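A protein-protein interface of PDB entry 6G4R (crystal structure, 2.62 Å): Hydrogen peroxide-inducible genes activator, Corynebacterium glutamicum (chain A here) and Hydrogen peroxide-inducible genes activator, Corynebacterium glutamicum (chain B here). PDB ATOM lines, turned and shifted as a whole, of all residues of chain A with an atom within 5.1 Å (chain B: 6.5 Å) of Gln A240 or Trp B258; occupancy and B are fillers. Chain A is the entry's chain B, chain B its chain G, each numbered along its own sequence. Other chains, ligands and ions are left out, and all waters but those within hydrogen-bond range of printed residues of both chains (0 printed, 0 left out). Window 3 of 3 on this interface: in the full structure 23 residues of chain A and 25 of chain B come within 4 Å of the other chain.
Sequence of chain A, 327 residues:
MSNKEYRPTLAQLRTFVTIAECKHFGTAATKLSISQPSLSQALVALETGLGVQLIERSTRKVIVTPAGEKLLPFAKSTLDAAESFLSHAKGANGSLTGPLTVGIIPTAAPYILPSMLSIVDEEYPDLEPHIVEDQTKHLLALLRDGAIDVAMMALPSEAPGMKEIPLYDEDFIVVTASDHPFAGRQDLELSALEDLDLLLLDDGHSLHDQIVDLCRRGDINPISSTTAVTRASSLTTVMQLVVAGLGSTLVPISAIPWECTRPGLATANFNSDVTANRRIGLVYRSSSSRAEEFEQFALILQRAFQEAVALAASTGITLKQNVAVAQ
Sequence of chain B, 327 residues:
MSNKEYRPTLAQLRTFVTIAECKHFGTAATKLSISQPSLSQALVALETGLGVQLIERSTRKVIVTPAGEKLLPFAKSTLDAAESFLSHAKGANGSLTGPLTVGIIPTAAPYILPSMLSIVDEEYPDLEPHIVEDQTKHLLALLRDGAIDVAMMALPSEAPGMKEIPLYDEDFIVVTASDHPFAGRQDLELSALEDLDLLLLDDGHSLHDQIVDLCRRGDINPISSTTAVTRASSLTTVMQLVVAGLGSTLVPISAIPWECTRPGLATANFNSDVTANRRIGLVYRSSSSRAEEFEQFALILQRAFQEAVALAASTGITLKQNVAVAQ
NE2 of Gln A240 is in hydrogen-bond range of O of Pro B110 (3.1 Å).
NH1 of Arg A262 sits close to NE2 of Gln A240 (3.0 Å).
Among the printed residues, pairs that only touch across the chains: Gln A240 with Pro B114, Gln A240 with Trp B258, Thr A237 with Pro B110, Thr A237 with Leu B113, Ala A244 with Leu B117, Leu A241 with Leu B113, Thr A236 with Pro B110 and Arg A262 with Trp B258.
Of chain B, only Pro B110 (3.1 Å), Pro B114 (3.2 Å) and Trp B258 (3.4 Å) come within 4 Å of Gln A240. Printed residues of chain A within 4 Å of Trp B258: Gln A240 (3.4 Å) and Arg A262 (3.99 Å). Printed residues of chain B within 4 Å of Thr A237: Pro B110 and Leu B113. Of the printed residues of chain A, Leu B113 touches Thr A237 (3.7 Å) and Leu A241 (3.8 Å). Of the printed residues of chain A, Leu B117 touches Ala A244 (3.7 Å). Of the printed residues of chain B, Thr A236 touches Pro B110 (3.8 Å). The nearest printed residue of chain A that does not touch Pro B114 is Ala A244 (6.1 Å).
Of the 10 printed residues of chain A, 6 touch a printed residue of chain B. Printed residues of chain A that touch a printed residue of chain B: Thr A236, Thr A237, Gln A240, Leu A241, Ala A244 and Arg A262. Hydrophobic or aromatic side chains of chain A that line the printed part of chain B: Leu A241 and Ala A244. Of the 18 printed residues of chain B, 5 touch a printed residue of chain A. Hydrophobic or aromatic side chains of chain B within 4 Å of the printed part of chain A: Pro B110, Leu B113, Pro B114, Leu B117 and Trp B258. Along chain B the printed residues that touch a printed residue of chain A span positions 110 to 258.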
ATOM      1  N   THR A 236     -11.030  -4.346  20.938  1.00  0.00           N
ATOM      2  CA  THR A 236     -11.256  -4.009  19.535  1.00  0.00           C
ATOM      3  C   THR A 236     -12.167  -2.795  19.385  1.00  0.00           C
ATOM      4  O   THR A 236     -12.028  -2.034  18.422  1.00  0.00           O
ATOM      5  CB  THR A 236     -11.833  -5.213  18.785  1.00  0.00           C
ATOM      6  OG1 THR A 236     -12.033  -4.871  17.408  1.00  0.00           O
ATOM      7  CG2 THR A 236     -13.156  -5.655  19.397  1.00  0.00           C
ATOM      8  N   THR A 237     -13.094  -2.589  20.323  1.00  0.00           N
ATOM      9  CA  THR A 237     -13.929  -1.393  20.278  1.00  0.00           C
ATOM     10  C   THR A 237     -13.142  -0.160  20.703  1.00  0.00           C
ATOM     11  O   THR A 237     -13.298   0.917  20.116  1.00  0.00           O
ATOM     12  CB  THR A 237     -15.164  -1.579  21.159  1.00  0.00           C
ATOM     13  OG1 THR A 237     -15.908  -2.717  20.705  1.00  0.00           O
ATOM     14  CG2 THR A 237     -16.054  -0.347  21.105  1.00  0.00           C
ATOM     15  N   VAL A 238     -12.295  -0.301  21.727  1.00  0.00           N
ATOM     16  CA  VAL A 238     -11.436   0.803  22.146  1.00  0.00           C
ATOM     17  C   VAL A 238     -10.528   1.235  21.002  1.00  0.00           C
ATOM     18  O   VAL A 238     -10.281   2.431  20.800  1.00  0.00           O
ATOM     19  CB  VAL A 238     -10.628   0.402  23.394  1.00  0.00           C
ATOM     20  CG1 VAL A 238      -9.573   1.449  23.712  1.00  0.00           C
ATOM     21  CG2 VAL A 238     -11.556   0.203  24.581  1.00  0.00           C
ATOM     22  N   MET A 239     -10.025   0.268  20.228  1.00  0.00           N
ATOM     23  CA  MET A 239      -9.129   0.589  19.120  1.00  0.00           C
ATOM     24  C   MET A 239      -9.815   1.468  18.081  1.00  0.00           C
ATOM     25  O   MET A 239      -9.204   2.401  17.548  1.00  0.00           O
ATOM     26  CB  MET A 239      -8.615  -0.697  18.473  1.00  0.00           C
ATOM     27  CG  MET A 239      -7.592  -1.435  19.309  1.00  0.00           C
ATOM     28  SD  MET A 239      -6.358  -0.315  19.988  1.00  0.00           S
ATOM     29  CE  MET A 239      -5.158  -1.483  20.608  1.00  0.00           C
ATOM     30  N   GLN A 240     -11.081   1.178  17.770  1.00  0.00           N
ATOM     31  CA  GLN A 240     -11.797   1.988  16.790  1.00  0.00           C
ATOM     32  C   GLN A 240     -11.989   3.419  17.277  1.00  0.00           C
ATOM     33  O   GLN A 240     -12.015   4.351  16.467  1.00  0.00           O
ATOM     34  CB  GLN A 240     -13.148   1.352  16.464  1.00  0.00           C
ATOM     35  CG  GLN A 240     -13.088  -0.135  16.125  1.00  0.00           C
ATOM     36  CD  GLN A 240     -12.424  -0.435  14.789  1.00  0.00           C
ATOM     37  OE1 GLN A 240     -11.819   0.435  14.163  1.00  0.00           O
ATOM     38  NE2 GLN A 240     -12.542  -1.681  14.347  1.00  0.00           N
ATOM     39  N   LEU A 241     -12.124   3.612  18.593  1.00  0.00           N
ATOM     40  CA  LEU A 241     -12.218   4.964  19.131  1.00  0.00           C
ATOM     41  C   LEU A 241     -10.885   5.694  19.042  1.00  0.00           C
ATOM     42  O   LEU A 241     -10.859   6.911  18.824  1.00  0.00           O
ATOM     43  CB  LEU A 241     -12.707   4.921  20.578  1.00  0.00           C
ATOM     44  CG  LEU A 241     -14.044   4.217  20.810  1.00  0.00           C
ATOM     45  CD1 LEU A 241     -14.414   4.243  22.283  1.00  0.00           C
ATOM     46  CD2 LEU A 241     -15.138   4.860  19.969  1.00  0.00           C
ATOM     47  N   VAL A 242      -9.774   4.974  19.207  1.00  0.00           N
ATOM     48  CA  VAL A 242      -8.460   5.605  19.119  1.00  0.00           C
ATOM     49  C   VAL A 242      -8.165   6.016  17.681  1.00  0.00           C
ATOM     50  O   VAL A 242      -7.559   7.068  17.434  1.00  0.00           O
ATOM     51  CB  VAL A 242      -7.378   4.665  19.679  1.00  0.00           C
ATOM     52  CG1 VAL A 242      -6.003   5.301  19.561  1.00  0.00           C
ATOM     53  CG2 VAL A 242      -7.679   4.323  21.130  1.00  0.00           C
ATOM     54  N   VAL A 243      -8.585   5.198  16.713  1.00  0.00           N
ATOM     55  CA  VAL A 243      -8.407   5.553  15.307  1.00  0.00           C
ATOM     56  C   VAL A 243      -9.163   6.835  14.984  1.00  0.00           C
ATOM     57  O   VAL A 243      -8.675   7.693  14.239  1.00  0.00           O
ATOM     58  CB  VAL A 243      -8.854   4.390  14.400  1.00  0.00           C
ATOM     59  CG1 VAL A 243      -8.847   4.815  12.942  1.00  0.00           C
ATOM     60  CG2 VAL A 243      -7.960   3.179  14.607  1.00  0.00           C
ATOM     61  N   ALA A 244     -10.358   6.994  15.551  1.00  0.00           N
ATOM     62  CA  ALA A 244     -11.168   8.183  15.320  1.00  0.00           C
ATOM     63  C   ALA A 244     -10.673   9.395  16.098  1.00  0.00           C
ATOM     64  O   ALA A 244     -11.265  10.473  15.973  1.00  0.00           O
ATOM     65  CB  ALA A 244     -12.630   7.900  15.680  1.00  0.00           C
ATOM     66  N   ARG A 262      -4.000  -2.337  12.531  1.00  0.00           N
ATOM     67  CA  ARG A 262      -4.935  -1.700  11.621  1.00  0.00           C
ATOM     68  C   ARG A 262      -4.469  -0.289  11.273  1.00  0.00           C
ATOM     69  O   ARG A 262      -3.718   0.335  12.027  1.00  0.00           O
ATOM     70  CB  ARG A 262      -6.326  -1.666  12.248  1.00  0.00           C
ATOM     71  CG  ARG A 262      -6.479  -0.666  13.380  1.00  0.00           C
ATOM     72  CD  ARG A 262      -7.746  -0.930  14.173  1.00  0.00           C
ATOM     73  NE  ARG A 262      -7.709  -2.233  14.829  1.00  0.00           N
ATOM     74  CZ  ARG A 262      -8.708  -2.742  15.542  1.00  0.00           C
ATOM     75  NH1 ARG A 262      -9.833  -2.056  15.694  1.00  0.00           N
ATOM     76  NH2 ARG A 262      -8.585  -3.937  16.102  1.00  0.00           N
ATOM     77  N   ALA B 109     -20.778  -2.936  17.739  1.00  0.00           N
ATOM     78  CA  ALA B 109     -20.023  -1.703  17.963  1.00  0.00           C
ATOM     79  C   ALA B 109     -18.734  -1.638  17.153  1.00  0.00           C
ATOM     80  O   ALA B 109     -18.586  -0.709  16.341  1.00  0.00           O
ATOM     81  CB  ALA B 109     -19.773  -1.525  19.464  1.00  0.00           C
ATOM     82  N   PRO B 110     -17.779  -2.567  17.295  1.00  0.00           N
ATOM     83  CA  PRO B 110     -16.481  -2.377  16.627  1.00  0.00           C
ATOM     84  C   PRO B 110     -16.549  -2.470  15.112  1.00  0.00           C
ATOM     85  O   PRO B 110     -15.562  -2.134  14.445  1.00  0.00           O
ATOM     86  CB  PRO B 110     -15.621  -3.503  17.209  1.00  0.00           C
ATOM     87  CG  PRO B 110     -16.593  -4.584  17.488  1.00  0.00           C
ATOM     88  CD  PRO B 110     -17.865  -3.900  17.924  1.00  0.00           C
ATOM     89  N   TYR B 111     -17.675  -2.908  14.551  1.00  0.00           N
ATOM     90  CA  TYR B 111     -17.825  -3.044  13.110  1.00  0.00           C
ATOM     91  C   TYR B 111     -18.608  -1.899  12.485  1.00  0.00           C
ATOM     92  O   TYR B 111     -18.535  -1.711  11.265  1.00  0.00           O
ATOM     93  CB  TYR B 111     -18.510  -4.377  12.786  1.00  0.00           C
ATOM     94  CG  TYR B 111     -17.999  -5.515  13.641  1.00  0.00           C
ATOM     95  CD1 TYR B 111     -16.636  -5.744  13.783  1.00  0.00           C
ATOM     96  CD2 TYR B 111     -18.877  -6.336  14.337  1.00  0.00           C
ATOM     97  CE1 TYR B 111     -16.162  -6.772  14.574  1.00  0.00           C
ATOM     98  CE2 TYR B 111     -18.412  -7.367  15.135  1.00  0.00           C
ATOM     99  CZ  TYR B 111     -17.053  -7.580  15.247  1.00  0.00           C
ATOM    100  OH  TYR B 111     -16.580  -8.603  16.035  1.00  0.00           O
ATOM    101  N   ILE B 112     -19.349  -1.137  13.288  1.00  0.00           N
ATOM    102  CA  ILE B 112     -20.077   0.025  12.797  1.00  0.00           C
ATOM    103  C   ILE B 112     -19.396   1.335  13.185  1.00  0.00           C
ATOM    104  O   ILE B 112     -19.626   2.358  12.523  1.00  0.00           O
ATOM    105  CB  ILE B 112     -21.538   0.010  13.300  1.00  0.00           C
ATOM    106  CG1 ILE B 112     -22.427   0.872  12.405  1.00  0.00           C
ATOM    107  CG2 ILE B 112     -21.621   0.485  14.745  1.00  0.00           C
ATOM    108  CD1 ILE B 112     -22.788   0.212  11.102  1.00  0.00           C
ATOM    109  N   LEU B 113     -18.559   1.331  14.225  1.00  0.00           N
ATOM    110  CA  LEU B 113     -17.946   2.569  14.703  1.00  0.00           C
ATOM    111  C   LEU B 113     -17.001   3.218  13.698  1.00  0.00           C
ATOM    112  O   LEU B 113     -17.097   4.443  13.511  1.00  0.00           O
ATOM    113  CB  LEU B 113     -17.232   2.305  16.033  1.00  0.00           C
ATOM    114  CG  LEU B 113     -18.101   2.253  17.291  1.00  0.00           C
ATOM    115  CD1 LEU B 113     -17.242   2.009  18.520  1.00  0.00           C
ATOM    116  CD2 LEU B 113     -18.915   3.524  17.445  1.00  0.00           C
ATOM    117  N   PRO B 114     -16.081   2.497  13.033  1.00  0.00           N
ATOM    118  CA  PRO B 114     -15.123   3.191  12.148  1.00  0.00           C
ATOM    119  C   PRO B 114     -15.779   4.086  11.112  1.00  0.00           C
ATOM    120  O   PRO B 114     -15.374   5.243  10.941  1.00  0.00           O
ATOM    121  CB  PRO B 114     -14.358   2.034  11.495  1.00  0.00           C
ATOM    122  CG  PRO B 114     -14.465   0.924  12.451  1.00  0.00           C
ATOM    123  CD  PRO B 114     -15.815   1.047  13.079  1.00  0.00           C
ATOM    124  N   LEU B 117     -18.012   7.081  13.126  1.00  0.00           N
ATOM    125  CA  LEU B 117     -17.277   8.233  13.640  1.00  0.00           C
ATOM    126  C   LEU B 117     -16.649   9.048  12.517  1.00  0.00           C
ATOM    127  O   LEU B 117     -16.476  10.263  12.660  1.00  0.00           O
ATOM    128  CB  LEU B 117     -16.200   7.799  14.639  1.00  0.00           C
ATOM    129  CG  LEU B 117     -16.595   7.303  16.036  1.00  0.00           C
ATOM    130  CD1 LEU B 117     -18.048   7.632  16.371  1.00  0.00           C
ATOM    131  CD2 LEU B 117     -16.310   5.820  16.215  1.00  0.00           C
ATOM    132  N   SER B 254     -20.804  -7.751   8.833  1.00  0.00           N
ATOM    133  CA  SER B 254     -19.964  -6.587   9.096  1.00  0.00           C
ATOM    134  C   SER B 254     -18.701  -6.941   9.871  1.00  0.00           C
ATOM    135  O   SER B 254     -17.751  -6.151   9.877  1.00  0.00           O
ATOM    136  CB  SER B 254     -20.755  -5.521   9.857  1.00  0.00           C
ATOM    137  OG  SER B 254     -21.145  -5.989  11.136  1.00  0.00           O
ATOM    138  N   ALA B 255     -18.668  -8.103  10.522  1.00  0.00           N
ATOM    139  CA  ALA B 255     -17.494  -8.545  11.264  1.00  0.00           C
ATOM    140  C   ALA B 255     -16.464  -9.245  10.388  1.00  0.00           C
ATOM    141  O   ALA B 255     -15.396  -9.611  10.892  1.00  0.00           O
ATOM    142  CB  ALA B 255     -17.914  -9.477  12.403  1.00  0.00           C
ATOM    143  N   ILE B 256     -16.760  -9.441   9.102  1.00  0.00           N
ATOM    144  CA  ILE B 256     -15.862 -10.214   8.241  1.00  0.00           C
ATOM    145  C   ILE B 256     -14.485  -9.573   8.102  1.00  0.00           C
ATOM    146  O   ILE B 256     -13.482 -10.270   8.324  1.00  0.00           O
ATOM    147  CB  ILE B 256     -16.536 -10.479   6.879  1.00  0.00           C
ATOM    148  CG1 ILE B 256     -17.642 -11.526   7.032  1.00  0.00           C
ATOM    149  CG2 ILE B 256     -15.508 -10.909   5.847  1.00  0.00           C
ATOM    150  CD1 ILE B 256     -18.527 -11.659   5.816  1.00  0.00           C
ATOM    151  N   PRO B 257     -14.352  -8.287   7.742  1.00  0.00           N
ATOM    152  CA  PRO B 257     -12.999  -7.728   7.568  1.00  0.00           C
ATOM    153  C   PRO B 257     -12.189  -7.673   8.851  1.00  0.00           C
ATOM    154  O   PRO B 257     -10.958  -7.576   8.781  1.00  0.00           O
ATOM    155  CB  PRO B 257     -13.264  -6.315   7.025  1.00  0.00           C
ATOM    156  CG  PRO B 257     -14.657  -6.350   6.511  1.00  0.00           C
ATOM    157  CD  PRO B 257     -15.384  -7.288   7.416  1.00  0.00           C
ATOM    158  N   TRP B 258     -12.833  -7.732  10.017  1.00  0.00           N
ATOM    159  CA  TRP B 258     -12.135  -7.585  11.287  1.00  0.00           C
ATOM    160  C   TRP B 258     -11.886  -8.903  12.007  1.00  0.00           C
ATOM    161  O   TRP B 258     -11.014  -8.953  12.881  1.00  0.00           O
ATOM    162  CB  TRP B 258     -12.921  -6.650  12.214  1.00  0.00           C
ATOM    163  CG  TRP B 258     -13.231  -5.319  11.598  1.00  0.00           C
ATOM    164  CD1 TRP B 258     -14.385  -4.960  10.962  1.00  0.00           C
ATOM    165  CD2 TRP B 258     -12.377  -4.170  11.561  1.00  0.00           C
ATOM    166  NE1 TRP B 258     -14.301  -3.658  10.531  1.00  0.00           N
ATOM    167  CE2 TRP B 258     -13.078  -3.151  10.886  1.00  0.00           C
ATOM    168  CE3 TRP B 258     -11.088  -3.904  12.032  1.00  0.00           C
ATOM    169  CZ2 TRP B 258     -12.533  -1.887  10.671  1.00  0.00           C
ATOM    170  CZ3 TRP B 258     -10.548  -2.650  11.817  1.00  0.00           C
ATOM    171  CH2 TRP B 258     -11.270  -1.657  11.142  1.00  0.00           C
ATOM    172  N   GLU B 259     -12.623  -9.963  11.674  1.00  0.00           N
ATOM    173  CA  GLU B 259     -12.503 -11.230  12.385  1.00  0.00           C
ATOM    174  C   GLU B 259     -12.283 -12.446  11.495  1.00  0.00           C
ATOM    175  O   GLU B 259     -11.820 -13.472  12.006  1.00  0.00           O
ATOM    176  CB  GLU B 259     -13.753 -11.483  13.246  1.00  0.00           C
ATOM    177  CG  GLU B 259     -14.176 -10.313  14.126  1.00  0.00           C
ATOM    178  CD  GLU B 259     -13.196 -10.032  15.250  1.00  0.00           C
ATOM    179  OE1 GLU B 259     -12.448 -10.956  15.635  1.00  0.00           O
ATOM    180  OE2 GLU B 259     -13.178  -8.889  15.752  1.00  0.00           O
ATOM    181  N   CYS B 260     -12.589 -12.377  10.199  1.00  0.00           N
ATOM    182  CA  CYS B 260     -12.598 -13.557   9.342  1.00  0.00           C
ATOM    183  C   CYS B 260     -11.489 -13.546   8.294  1.00  0.00           C
ATOM    184  O   CYS B 260     -11.566 -14.294   7.315  1.00  0.00           O
ATOM    185  CB  CYS B 260     -13.957 -13.701   8.655  1.00  0.00           C
ATOM    186  SG  CYS B 260     -15.373 -13.749   9.775  1.00  0.00           S
ATOM    187  N   THR B 261     -10.457 -12.723   8.473  1.00  0.00           N
ATOM    188  CA  THR B 261      -9.371 -12.649   7.506  1.00  0.00           C
ATOM    189  C   THR B 261      -8.044 -13.165   8.048  1.00  0.00           C
ATOM    190  O   THR B 261      -7.038 -13.114   7.332  1.00  0.00           O
ATOM    191  CB  THR B 261      -9.196 -11.209   7.008  1.00  0.00           C
ATOM    192  OG1 THR B 261      -8.852 -10.357   8.108  1.00  0.00           O
ATOM    193  CG2 THR B 261     -10.481 -10.710   6.365  1.00  0.00           C
ATOM    194  N   ARG B 262      -8.013 -13.663   9.278  1.00  0.00           N
ATOM    195  CA  ARG B 262      -6.803 -14.271   9.802  1.00  0.00           C
ATOM    196  C   ARG B 262      -6.650 -15.677   9.227  1.00  0.00           C
ATOM    197  O   ARG B 262      -7.630 -16.290   8.796  1.00  0.00           O
ATOM    198  CB  ARG B 262      -6.848 -14.300  11.329  1.00  0.00           C
ATOM    199  CG  ARG B 262      -7.789 -15.332  11.899  1.00  0.00           C
ATOM    200  CD  ARG B 262      -8.084 -15.111  13.372  1.00  0.00           C
ATOM    201  NE  ARG B 262      -8.792 -13.857  13.607  1.00  0.00           N
ATOM    202  CZ  ARG B 262      -9.133 -13.407  14.810  1.00  0.00           C
ATOM    203  NH1 ARG B 262      -8.830 -14.110  15.893  1.00  0.00           N
ATOM    204  NH2 ARG B 262      -9.778 -12.255  14.932  1.00  0.00           N
ATOM    205  N   ALA B 308     -19.812  -0.448   5.809  1.00  0.00           N
ATOM    206  CA  ALA B 308     -19.255  -1.650   6.422  1.00  0.00           C
ATOM    207  C   ALA B 308     -19.495  -2.878   5.553  1.00  0.00           C
ATOM    208  O   ALA B 308     -18.642  -3.770   5.479  1.00  0.00           O
ATOM    209  CB  ALA B 308     -19.849  -1.853   7.816  1.00  0.00           C
ATOM    210  N   LEU B 311     -17.016  -2.793   2.743  1.00  0.00           N
ATOM    211  CA  LEU B 311     -15.709  -3.260   3.196  1.00  0.00           C
ATOM    212  C   LEU B 311     -15.666  -4.780   3.269  1.00  0.00           C
ATOM    213  O   LEU B 311     -14.637  -5.396   2.965  1.00  0.00           O
ATOM    214  CB  LEU B 311     -15.375  -2.645   4.555  1.00  0.00           C
ATOM    215  CG  LEU B 311     -13.965  -2.915   5.086  1.00  0.00           C
ATOM    216  CD1 LEU B 311     -12.924  -2.275   4.182  1.00  0.00           C
ATOM    217  CD2 LEU B 311     -13.821  -2.416   6.516  1.00  0.00           C
